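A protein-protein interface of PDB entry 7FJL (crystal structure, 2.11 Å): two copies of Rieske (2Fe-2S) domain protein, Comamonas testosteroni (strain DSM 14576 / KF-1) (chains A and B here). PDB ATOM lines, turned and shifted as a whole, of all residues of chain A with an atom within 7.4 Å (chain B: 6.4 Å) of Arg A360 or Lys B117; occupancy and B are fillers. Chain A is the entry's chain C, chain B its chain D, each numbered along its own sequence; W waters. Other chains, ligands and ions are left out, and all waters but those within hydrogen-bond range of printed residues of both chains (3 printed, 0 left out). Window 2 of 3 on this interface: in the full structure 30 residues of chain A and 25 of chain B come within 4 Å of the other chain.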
ATOM      1  N   MET A   1       5.249 -17.482   3.145  1.00  0.00           N
ATOM      2  CA  MET A   1       6.175 -16.441   3.721  1.00  0.00           C
ATOM      3  C   MET A   1       5.755 -16.053   5.136  1.00  0.00           C
ATOM      4  O   MET A   1       4.745 -15.368   5.296  1.00  0.00           O
ATOM      5  CB  MET A   1       6.108 -15.164   2.883  1.00  0.00           C
ATOM      6  CG  MET A   1       7.461 -14.558   2.557  1.00  0.00           C
ATOM      7  SD  MET A   1       8.744 -15.836   2.337  1.00  0.00           S
ATOM      8  CE  MET A   1      10.146 -15.039   3.136  1.00  0.00           C
ATOM      9  N   ARG A 356      13.018 -15.253   9.872  1.00  0.00           N
ATOM     10  CA  ARG A 356      12.372 -16.161   8.919  1.00  0.00           C
ATOM     11  C   ARG A 356      11.557 -15.431   7.836  1.00  0.00           C
ATOM     12  O   ARG A 356      11.132 -15.992   6.838  1.00  0.00           O
ATOM     13  CB  ARG A 356      11.434 -17.068   9.716  1.00  0.00           C
ATOM     14  CG  ARG A 356      12.196 -18.112  10.509  1.00  0.00           C
ATOM     15  CD  ARG A 356      11.212 -18.883  11.396  1.00  0.00           C
ATOM     16  NE  ARG A 356      12.132 -19.741  12.135  1.00  0.00           N
ATOM     17  CZ  ARG A 356      12.878 -19.315  13.200  1.00  0.00           C
ATOM     18  NH1 ARG A 356      12.774 -18.069  13.673  1.00  0.00           N
ATOM     19  NH2 ARG A 356      13.752 -20.150  13.759  1.00  0.00           N
ATOM     20  N   THR A 357      11.388 -14.139   7.998  1.00  0.00           N
ATOM     21  CA  THR A 357      10.779 -13.272   7.005  1.00  0.00           C
ATOM     22  C   THR A 357      11.651 -13.121   5.764  1.00  0.00           C
ATOM     23  O   THR A 357      11.212 -12.578   4.762  1.00  0.00           O
ATOM     24  CB  THR A 357      10.672 -11.948   7.752  1.00  0.00           C
ATOM     25  OG1 THR A 357       9.425 -11.915   8.448  1.00  0.00           O
ATOM     26  CG2 THR A 357      11.165 -10.754   6.999  1.00  0.00           C
ATOM     27  N   HIS A 358      12.907 -13.559   5.851  1.00  0.00           N
ATOM     28  CA  HIS A 358      13.868 -13.311   4.800  1.00  0.00           C
ATOM     29  C   HIS A 358      14.396 -14.618   4.233  1.00  0.00           C
ATOM     30  O   HIS A 358      15.384 -14.585   3.500  1.00  0.00           O
ATOM     31  CB  HIS A 358      14.999 -12.417   5.316  1.00  0.00           C
ATOM     32  CG  HIS A 358      14.574 -10.992   5.485  1.00  0.00           C
ATOM     33  ND1 HIS A 358      14.081 -10.227   4.418  1.00  0.00           N
ATOM     34  CD2 HIS A 358      14.513 -10.205   6.591  1.00  0.00           C
ATOM     35  CE1 HIS A 358      13.755  -9.024   4.862  1.00  0.00           C
ATOM     36  NE2 HIS A 358      13.995  -8.997   6.208  1.00  0.00           N
ATOM     37  N   ASP A 359      13.749 -15.742   4.585  1.00  0.00           N
ATOM     38  CA  ASP A 359      14.166 -17.073   4.153  1.00  0.00           C
ATOM     39  C   ASP A 359      13.729 -17.268   2.710  1.00  0.00           C
ATOM     40  O   ASP A 359      12.790 -16.638   2.245  1.00  0.00           O
ATOM     41  CB  ASP A 359      13.511 -18.200   4.961  1.00  0.00           C
ATOM     42  CG  ASP A 359      14.037 -18.443   6.380  1.00  0.00           C
ATOM     43  OD1 ASP A 359      15.076 -17.846   6.796  1.00  0.00           O
ATOM     44  OD2 ASP A 359      13.385 -19.203   7.089  1.00  0.00           O
ATOM     45  N   ARG A 360      14.404 -18.181   2.031  1.00  0.00           N
ATOM     46  CA  ARG A 360      14.027 -18.623   0.709  1.00  0.00           C
ATOM     47  C   ARG A 360      14.083 -20.144   0.721  1.00  0.00           C
ATOM     48  O   ARG A 360      15.090 -20.721   0.316  1.00  0.00           O
ATOM     49  CB  ARG A 360      15.092 -18.123  -0.267  1.00  0.00           C
ATOM     50  CG  ARG A 360      14.584 -17.250  -1.379  1.00  0.00           C
ATOM     51  CD  ARG A 360      14.466 -15.766  -1.125  1.00  0.00           C
ATOM     52  NE  ARG A 360      14.383 -15.228  -2.491  1.00  0.00           N
ATOM     53  CZ  ARG A 360      13.790 -15.838  -3.534  1.00  0.00           C
ATOM     54  NH1 ARG A 360      13.163 -17.007  -3.405  1.00  0.00           N
ATOM     55  NH2 ARG A 360      13.814 -15.260  -4.719  1.00  0.00           N
ATOM     56  N   LEU A 361      13.044 -20.785   1.240  1.00  0.00           N
ATOM     57  CA  LEU A 361      13.095 -22.199   1.563  1.00  0.00           C
ATOM     58  C   LEU A 361      12.977 -23.033   0.292  1.00  0.00           C
ATOM     59  O   LEU A 361      12.561 -22.533  -0.739  1.00  0.00           O
ATOM     60  CB  LEU A 361      11.948 -22.500   2.524  1.00  0.00           C
ATOM     61  CG  LEU A 361      12.047 -21.783   3.878  1.00  0.00           C
ATOM     62  CD1 LEU A 361      11.057 -22.390   4.863  1.00  0.00           C
ATOM     63  CD2 LEU A 361      13.467 -21.853   4.450  1.00  0.00           C
ATOM     64  N   GLY A 362      13.345 -24.318   0.367  1.00  0.00           N
ATOM     65  CA  GLY A 362      13.338 -25.184  -0.811  1.00  0.00           C
ATOM     66  C   GLY A 362      12.770 -26.539  -0.433  1.00  0.00           C
ATOM     67  O   GLY A 362      12.274 -26.677   0.680  1.00  0.00           O
ATOM     68  N   ALA A 363      12.817 -27.504  -1.366  1.00  0.00           N
ATOM     69  CA  ALA A 363      12.415 -28.883  -1.115  1.00  0.00           C
ATOM     70  C   ALA A 363      13.024 -29.387   0.188  1.00  0.00           C
ATOM     71  O   ALA A 363      12.340 -30.064   0.957  1.00  0.00           O
ATOM     72  CB  ALA A 363      12.755 -29.793  -2.273  1.00  0.00           C
ATOM     73  N   ASP A 365      13.606 -27.910   2.829  1.00  0.00           N
ATOM     74  CA  ASP A 365      13.048 -27.293   4.015  1.00  0.00           C
ATOM     75  C   ASP A 365      11.702 -27.883   4.465  1.00  0.00           C
ATOM     76  O   ASP A 365      11.039 -27.334   5.372  1.00  0.00           O
ATOM     77  CB  ASP A 365      13.049 -25.770   3.878  1.00  0.00           C
ATOM     78  CG  ASP A 365      14.485 -25.283   3.664  1.00  0.00           C
ATOM     79  OD1 ASP A 365      14.772 -24.931   2.518  1.00  0.00           O
ATOM     80  OD2 ASP A 365      15.320 -25.327   4.634  1.00  0.00           O
ATOM     81  N   ARG A 372       7.242 -25.008  11.418  1.00  0.00           N
ATOM     82  CA  ARG A 372       6.768 -23.638  11.545  1.00  0.00           C
ATOM     83  C   ARG A 372       5.228 -23.608  11.542  1.00  0.00           C
ATOM     84  O   ARG A 372       4.620 -23.043  12.484  1.00  0.00           O
ATOM     85  CB  ARG A 372       7.364 -22.714  10.478  1.00  0.00           C
ATOM     86  CG  ARG A 372       8.880 -22.618  10.534  1.00  0.00           C
ATOM     87  CD  ARG A 372       9.485 -22.018   9.273  1.00  0.00           C
ATOM     88  NE  ARG A 372      10.884 -21.881   9.614  1.00  0.00           N
ATOM     89  CZ  ARG A 372      11.776 -21.232   8.859  1.00  0.00           C
ATOM     90  NH1 ARG A 372      11.377 -20.588   7.769  1.00  0.00           N
ATOM     91  NH2 ARG A 372      13.034 -21.117   9.263  1.00  0.00           N
ATOM     92  N   PRO B  71      21.288 -16.405   0.886  1.00  0.00           N
ATOM     93  CA  PRO B  71      19.866 -16.185   0.573  1.00  0.00           C
ATOM     94  C   PRO B  71      18.944 -17.336   0.974  1.00  0.00           C
ATOM     95  O   PRO B  71      17.746 -17.137   0.977  1.00  0.00           O
ATOM     96  CB  PRO B  71      19.836 -15.997  -0.948  1.00  0.00           C
ATOM     97  CG  PRO B  71      21.031 -16.818  -1.377  1.00  0.00           C
ATOM     98  CD  PRO B  71      22.118 -16.489  -0.347  1.00  0.00           C
ATOM     99  N   HIS B  72      19.478 -18.526   1.297  1.00  0.00           N
ATOM    100  CA  HIS B  72      18.685 -19.650   1.794  1.00  0.00           C
ATOM    101  C   HIS B  72      18.120 -19.422   3.209  1.00  0.00           C
ATOM    102  O   HIS B  72      16.940 -19.074   3.336  1.00  0.00           O
ATOM    103  CB  HIS B  72      19.480 -20.960   1.685  1.00  0.00           C
ATOM    104  CG  HIS B  72      18.715 -22.148   2.138  1.00  0.00           C
ATOM    105  ND1 HIS B  72      19.343 -23.231   2.734  1.00  0.00           N
ATOM    106  CD2 HIS B  72      17.377 -22.446   2.097  1.00  0.00           C
ATOM    107  CE1 HIS B  72      18.452 -24.166   3.022  1.00  0.00           C
ATOM    108  NE2 HIS B  72      17.214 -23.713   2.656  1.00  0.00           N
ATOM    109  N   ARG B  73      18.911 -19.676   4.273  1.00  0.00           N
ATOM    110  CA  ARG B  73      18.474 -19.391   5.635  1.00  0.00           C
ATOM    111  C   ARG B  73      19.406 -18.410   6.394  1.00  0.00           C
ATOM    112  O   ARG B  73      19.382 -18.364   7.647  1.00  0.00           O
ATOM    113  CB  ARG B  73      18.214 -20.697   6.397  1.00  0.00           C
ATOM    114  CG  ARG B  73      17.200 -21.655   5.763  1.00  0.00           C
ATOM    115  CD  ARG B  73      16.313 -22.225   6.889  1.00  0.00           C
ATOM    116  NE  ARG B  73      16.938 -23.045   7.932  1.00  0.00           N
ATOM    117  CZ  ARG B  73      17.434 -24.280   7.801  1.00  0.00           C
ATOM    118  NH1 ARG B  73      17.349 -24.952   6.664  1.00  0.00           N
ATOM    119  NH2 ARG B  73      18.010 -24.865   8.843  1.00  0.00           N
ATOM    120  N   TRP B  94      24.487 -24.065  -1.110  1.00  0.00           N
ATOM    121  CA  TRP B  94      24.208 -23.057  -2.132  1.00  0.00           C
ATOM    122  C   TRP B  94      25.463 -22.300  -2.501  1.00  0.00           C
ATOM    123  O   TRP B  94      26.223 -21.862  -1.610  1.00  0.00           O
ATOM    124  CB  TRP B  94      23.170 -22.030  -1.634  1.00  0.00           C
ATOM    125  CG  TRP B  94      21.775 -22.560  -1.506  1.00  0.00           C
ATOM    126  CD1 TRP B  94      21.387 -23.843  -1.227  1.00  0.00           C
ATOM    127  CD2 TRP B  94      20.568 -21.805  -1.629  1.00  0.00           C
ATOM    128  NE1 TRP B  94      20.033 -23.905  -1.090  1.00  0.00           N
ATOM    129  CE2 TRP B  94      19.495 -22.696  -1.405  1.00  0.00           C
ATOM    130  CE3 TRP B  94      20.293 -20.479  -1.962  1.00  0.00           C
ATOM    131  CZ2 TRP B  94      18.161 -22.297  -1.443  1.00  0.00           C
ATOM    132  CZ3 TRP B  94      18.968 -20.084  -1.997  1.00  0.00           C
ATOM    133  CH2 TRP B  94      17.931 -20.972  -1.714  1.00  0.00           C
ATOM    134  N   MET B 105      22.585 -25.531  -6.030  1.00  0.00           N
ATOM    135  CA  MET B 105      22.006 -25.784  -4.720  1.00  0.00           C
ATOM    136  C   MET B 105      22.238 -27.248  -4.359  1.00  0.00           C
ATOM    137  O   MET B 105      21.578 -28.150  -4.887  1.00  0.00           O
ATOM    138  CB  MET B 105      20.504 -25.461  -4.732  1.00  0.00           C
ATOM    139  CG  MET B 105      20.202 -23.958  -4.833  1.00  0.00           C
ATOM    140  SD  MET B 105      18.447 -23.567  -5.003  1.00  0.00           S
ATOM    141  CE  MET B 105      18.517 -21.832  -5.488  1.00  0.00           C
ATOM    142  N   SER B 112      12.569 -28.744 -10.018  1.00  0.00           N
ATOM    143  CA  SER B 112      11.988 -27.420  -9.807  1.00  0.00           C
ATOM    144  C   SER B 112      12.987 -26.298 -10.084  1.00  0.00           C
ATOM    145  O   SER B 112      14.052 -26.243  -9.474  1.00  0.00           O
ATOM    146  CB  SER B 112      11.418 -27.310  -8.421  1.00  0.00           C
ATOM    147  OG  SER B 112      10.492 -28.362  -8.189  1.00  0.00           O
ATOM    148  N   GLY B 113      12.608 -25.386 -10.990  1.00  0.00           N
ATOM    149  CA  GLY B 113      13.505 -24.370 -11.519  1.00  0.00           C
ATOM    150  C   GLY B 113      13.758 -23.233 -10.532  1.00  0.00           C
ATOM    151  O   GLY B 113      13.364 -22.092 -10.782  1.00  0.00           O
ATOM    152  N   MET B 114      14.440 -23.568  -9.425  1.00  0.00           N
ATOM    153  CA  MET B 114      14.622 -22.680  -8.283  1.00  0.00           C
ATOM    154  C   MET B 114      16.030 -22.069  -8.300  1.00  0.00           C
ATOM    155  O   MET B 114      16.253 -21.006  -7.710  1.00  0.00           O
ATOM    156  CB  MET B 114      14.363 -23.420  -6.960  1.00  0.00           C
ATOM    157  CG  MET B 114      13.922 -22.506  -5.816  1.00  0.00           C
ATOM    158  SD  MET B 114      14.413 -23.056  -4.145  1.00  0.00           S
ATOM    159  CE  MET B 114      14.089 -21.546  -3.234  1.00  0.00           C
ATOM    160  N   VAL B 115      16.961 -22.743  -9.003  1.00  0.00           N
ATOM    161  CA  VAL B 115      18.356 -22.336  -9.158  1.00  0.00           C
ATOM    162  C   VAL B 115      18.415 -20.968  -9.861  1.00  0.00           C
ATOM    163  O   VAL B 115      19.292 -20.151  -9.560  1.00  0.00           O
ATOM    164  CB  VAL B 115      19.189 -23.454  -9.844  1.00  0.00           C
ATOM    165  CG1 VAL B 115      20.582 -23.033 -10.290  1.00  0.00           C
ATOM    166  CG2 VAL B 115      19.291 -24.711  -8.991  1.00  0.00           C
ATOM    167  N   ASP B 116      17.427 -20.693 -10.736  1.00  0.00           N
ATOM    168  CA  ASP B 116      17.389 -19.504 -11.583  1.00  0.00           C
ATOM    169  C   ASP B 116      16.515 -18.400 -10.975  1.00  0.00           C
ATOM    170  O   ASP B 116      16.610 -17.241 -11.384  1.00  0.00           O
ATOM    171  CB  ASP B 116      16.964 -19.849 -13.018  1.00  0.00           C
ATOM    172  CG  ASP B 116      18.049 -20.463 -13.898  1.00  0.00           C
ATOM    173  OD1 ASP B 116      19.183 -20.659 -13.406  1.00  0.00           O
ATOM    174  OD2 ASP B 116      17.750 -20.740 -15.083  1.00  0.00           O
ATOM    175  N   LYS B 117      15.694 -18.759  -9.978  1.00  0.00           N
ATOM    176  CA  LYS B 117      14.707 -17.872  -9.376  1.00  0.00           C
ATOM    177  C   LYS B 117      15.313 -16.982  -8.289  1.00  0.00           C
ATOM    178  O   LYS B 117      14.762 -15.919  -8.012  1.00  0.00           O
ATOM    179  CB  LYS B 117      13.601 -18.706  -8.727  1.00  0.00           C
ATOM    180  CG  LYS B 117      12.173 -18.228  -8.945  1.00  0.00           C
ATOM    181  CD  LYS B 117      11.177 -19.298  -8.517  1.00  0.00           C
ATOM    182  CE  LYS B 117      11.357 -20.630  -9.219  1.00  0.00           C
ATOM    183  NZ  LYS B 117      11.242 -21.770  -8.278  1.00  0.00           N
ATOM    184  N   VAL B 118      16.377 -17.448  -7.612  1.00  0.00           N
ATOM    185  CA  VAL B 118      16.999 -16.690  -6.529  1.00  0.00           C
ATOM    186  C   VAL B 118      18.216 -15.961  -7.098  1.00  0.00           C
ATOM    187  O   VAL B 118      19.054 -16.550  -7.794  1.00  0.00           O
ATOM    188  CB  VAL B 118      17.404 -17.571  -5.323  1.00  0.00           C
ATOM    189  CG1 VAL B 118      17.975 -16.743  -4.178  1.00  0.00           C
ATOM    190  CG2 VAL B 118      16.267 -18.457  -4.848  1.00  0.00           C
ATOM    191  N   LYS B 119      18.276 -14.660  -6.823  1.00  0.00           N
ATOM    192  CA  LYS B 119      19.476 -13.891  -7.109  1.00  0.00           C
ATOM    193  C   LYS B 119      19.932 -13.218  -5.825  1.00  0.00           C
ATOM    194  O   LYS B 119      19.131 -12.576  -5.171  1.00  0.00           O
ATOM    195  CB  LYS B 119      19.224 -12.926  -8.262  1.00  0.00           C
ATOM    196  CG  LYS B 119      19.440 -13.548  -9.637  1.00  0.00           C
ATOM    197  CD  LYS B 119      19.930 -12.518 -10.656  1.00  0.00           C
ATOM    198  CE  LYS B 119      21.084 -11.676 -10.144  1.00  0.00           C
ATOM    199  NZ  LYS B 119      21.915 -11.148 -11.253  1.00  0.00           N
HETATM  200  O   HOH W   1      15.719 -13.314  -5.971  1.00  0.00           O
HETATM  201  O   HOH W   2      17.288 -27.006   4.213  1.00  0.00           O
HETATM  202  O   HOH W   3      16.790 -14.828   1.430  1.00  0.00           O
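The side-chain carboxylate of Asp A365 is in salt-bridge range of the guanidinium group of Arg B73, at 2.9 Å. The backbone NH of Arg A360 lies within hydrogen-bond range of the backbone carbonyl oxygen of His B72, at 3.0 Å. A ring nitrogen (NE2) of His B72 sits at hydrogen-bond distance from the side-chain carboxylate of Asp A365, at 2.7 Å. NH2 of Arg A360 is in hydrogen-bond range of O of Lys B117, at 3.5 Å.
The backbone NH of Gly A362 lies within hydrogen-bond range of the side-chain carboxylate of Asp A365. OD2 of Asp A359 is in salt-bridge range of NH1 of Arg A372 (2.5 Å). The backbone carbonyl oxygen (O) of Gly B113 lies close to the side-chain amino group (NZ) of Lys B117.
Asp A359 touches His B72. Arg B73 touches Asp A359 (CA to OD1, 3.9 Å). Pro B71 touches Arg A360. Trp B94 touches Arg A360. O of Arg A360 touches CE of Met B114, 3.8 Å away. Arg A360 touches Val B118. CD2 of Leu A361 touches CD of Arg B73 (3.8 Å). Leu A361 touches Met B114 (O to CE, 3.1 Å).
Arg A356 touches none of the printed residues of chain B. Of chain B, only Pro B71 (3.1 Å), His B72 (3.0 Å), Trp B94 (3.5 Å), Met B114 (3.8 Å), Lys B117 (3.5 Å) and Val B118 (3.7 Å) come within 4 Å of Arg A360. Of the printed residues of chain B, Asp A365 touches His B72 and Arg B73. Arg A372 touches none of the printed residues of chain B. Of the printed residues of chain A, Pro B71 touches Arg A360 (3.1 Å). Of the printed residues of chain A, Arg B73 touches Asp A359, Leu A361 and Asp A365. Of chain A, only Arg A360 comes within 4 Å of Lys B117. Of the printed residues of chain A, Val B118 touches Arg A360. The nearest printed residue of chain A that does not touch Lys B117 is Leu A361 (7.7 Å). The nearest printed residue of chain B that does not touch Leu A361 is His B72 (4.3 Å).
Of the 11 printed residues of chain A, 4 touch a printed residue of chain B. Hydrophobic or aromatic side chains of chain A that line the printed part of chain B: Leu A361. Along chain A the printed residues that touch a printed residue of chain B span positions 359 to 365.
No position is printed for both chains. Of the 12 pairs that touch across the chains among the printed residues, none has its exchanged pair printed and touching as well.
Water W3 lies within hydrogen-bond range of the backbone carbonyl oxygen of His A358 (2.5 Å) and the backbone carbonyl oxygen of Pro B71 (2.5 Å). Water W2 lies within hydrogen-bond range of the side-chain carboxylate of Asp A365 (2.6 Å) and the guanidinium group of Arg B73 (3.2 Å). Water W1 lies within hydrogen-bond range of NH2 of Arg A360, N of Lys B119 and O of Lys B117.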
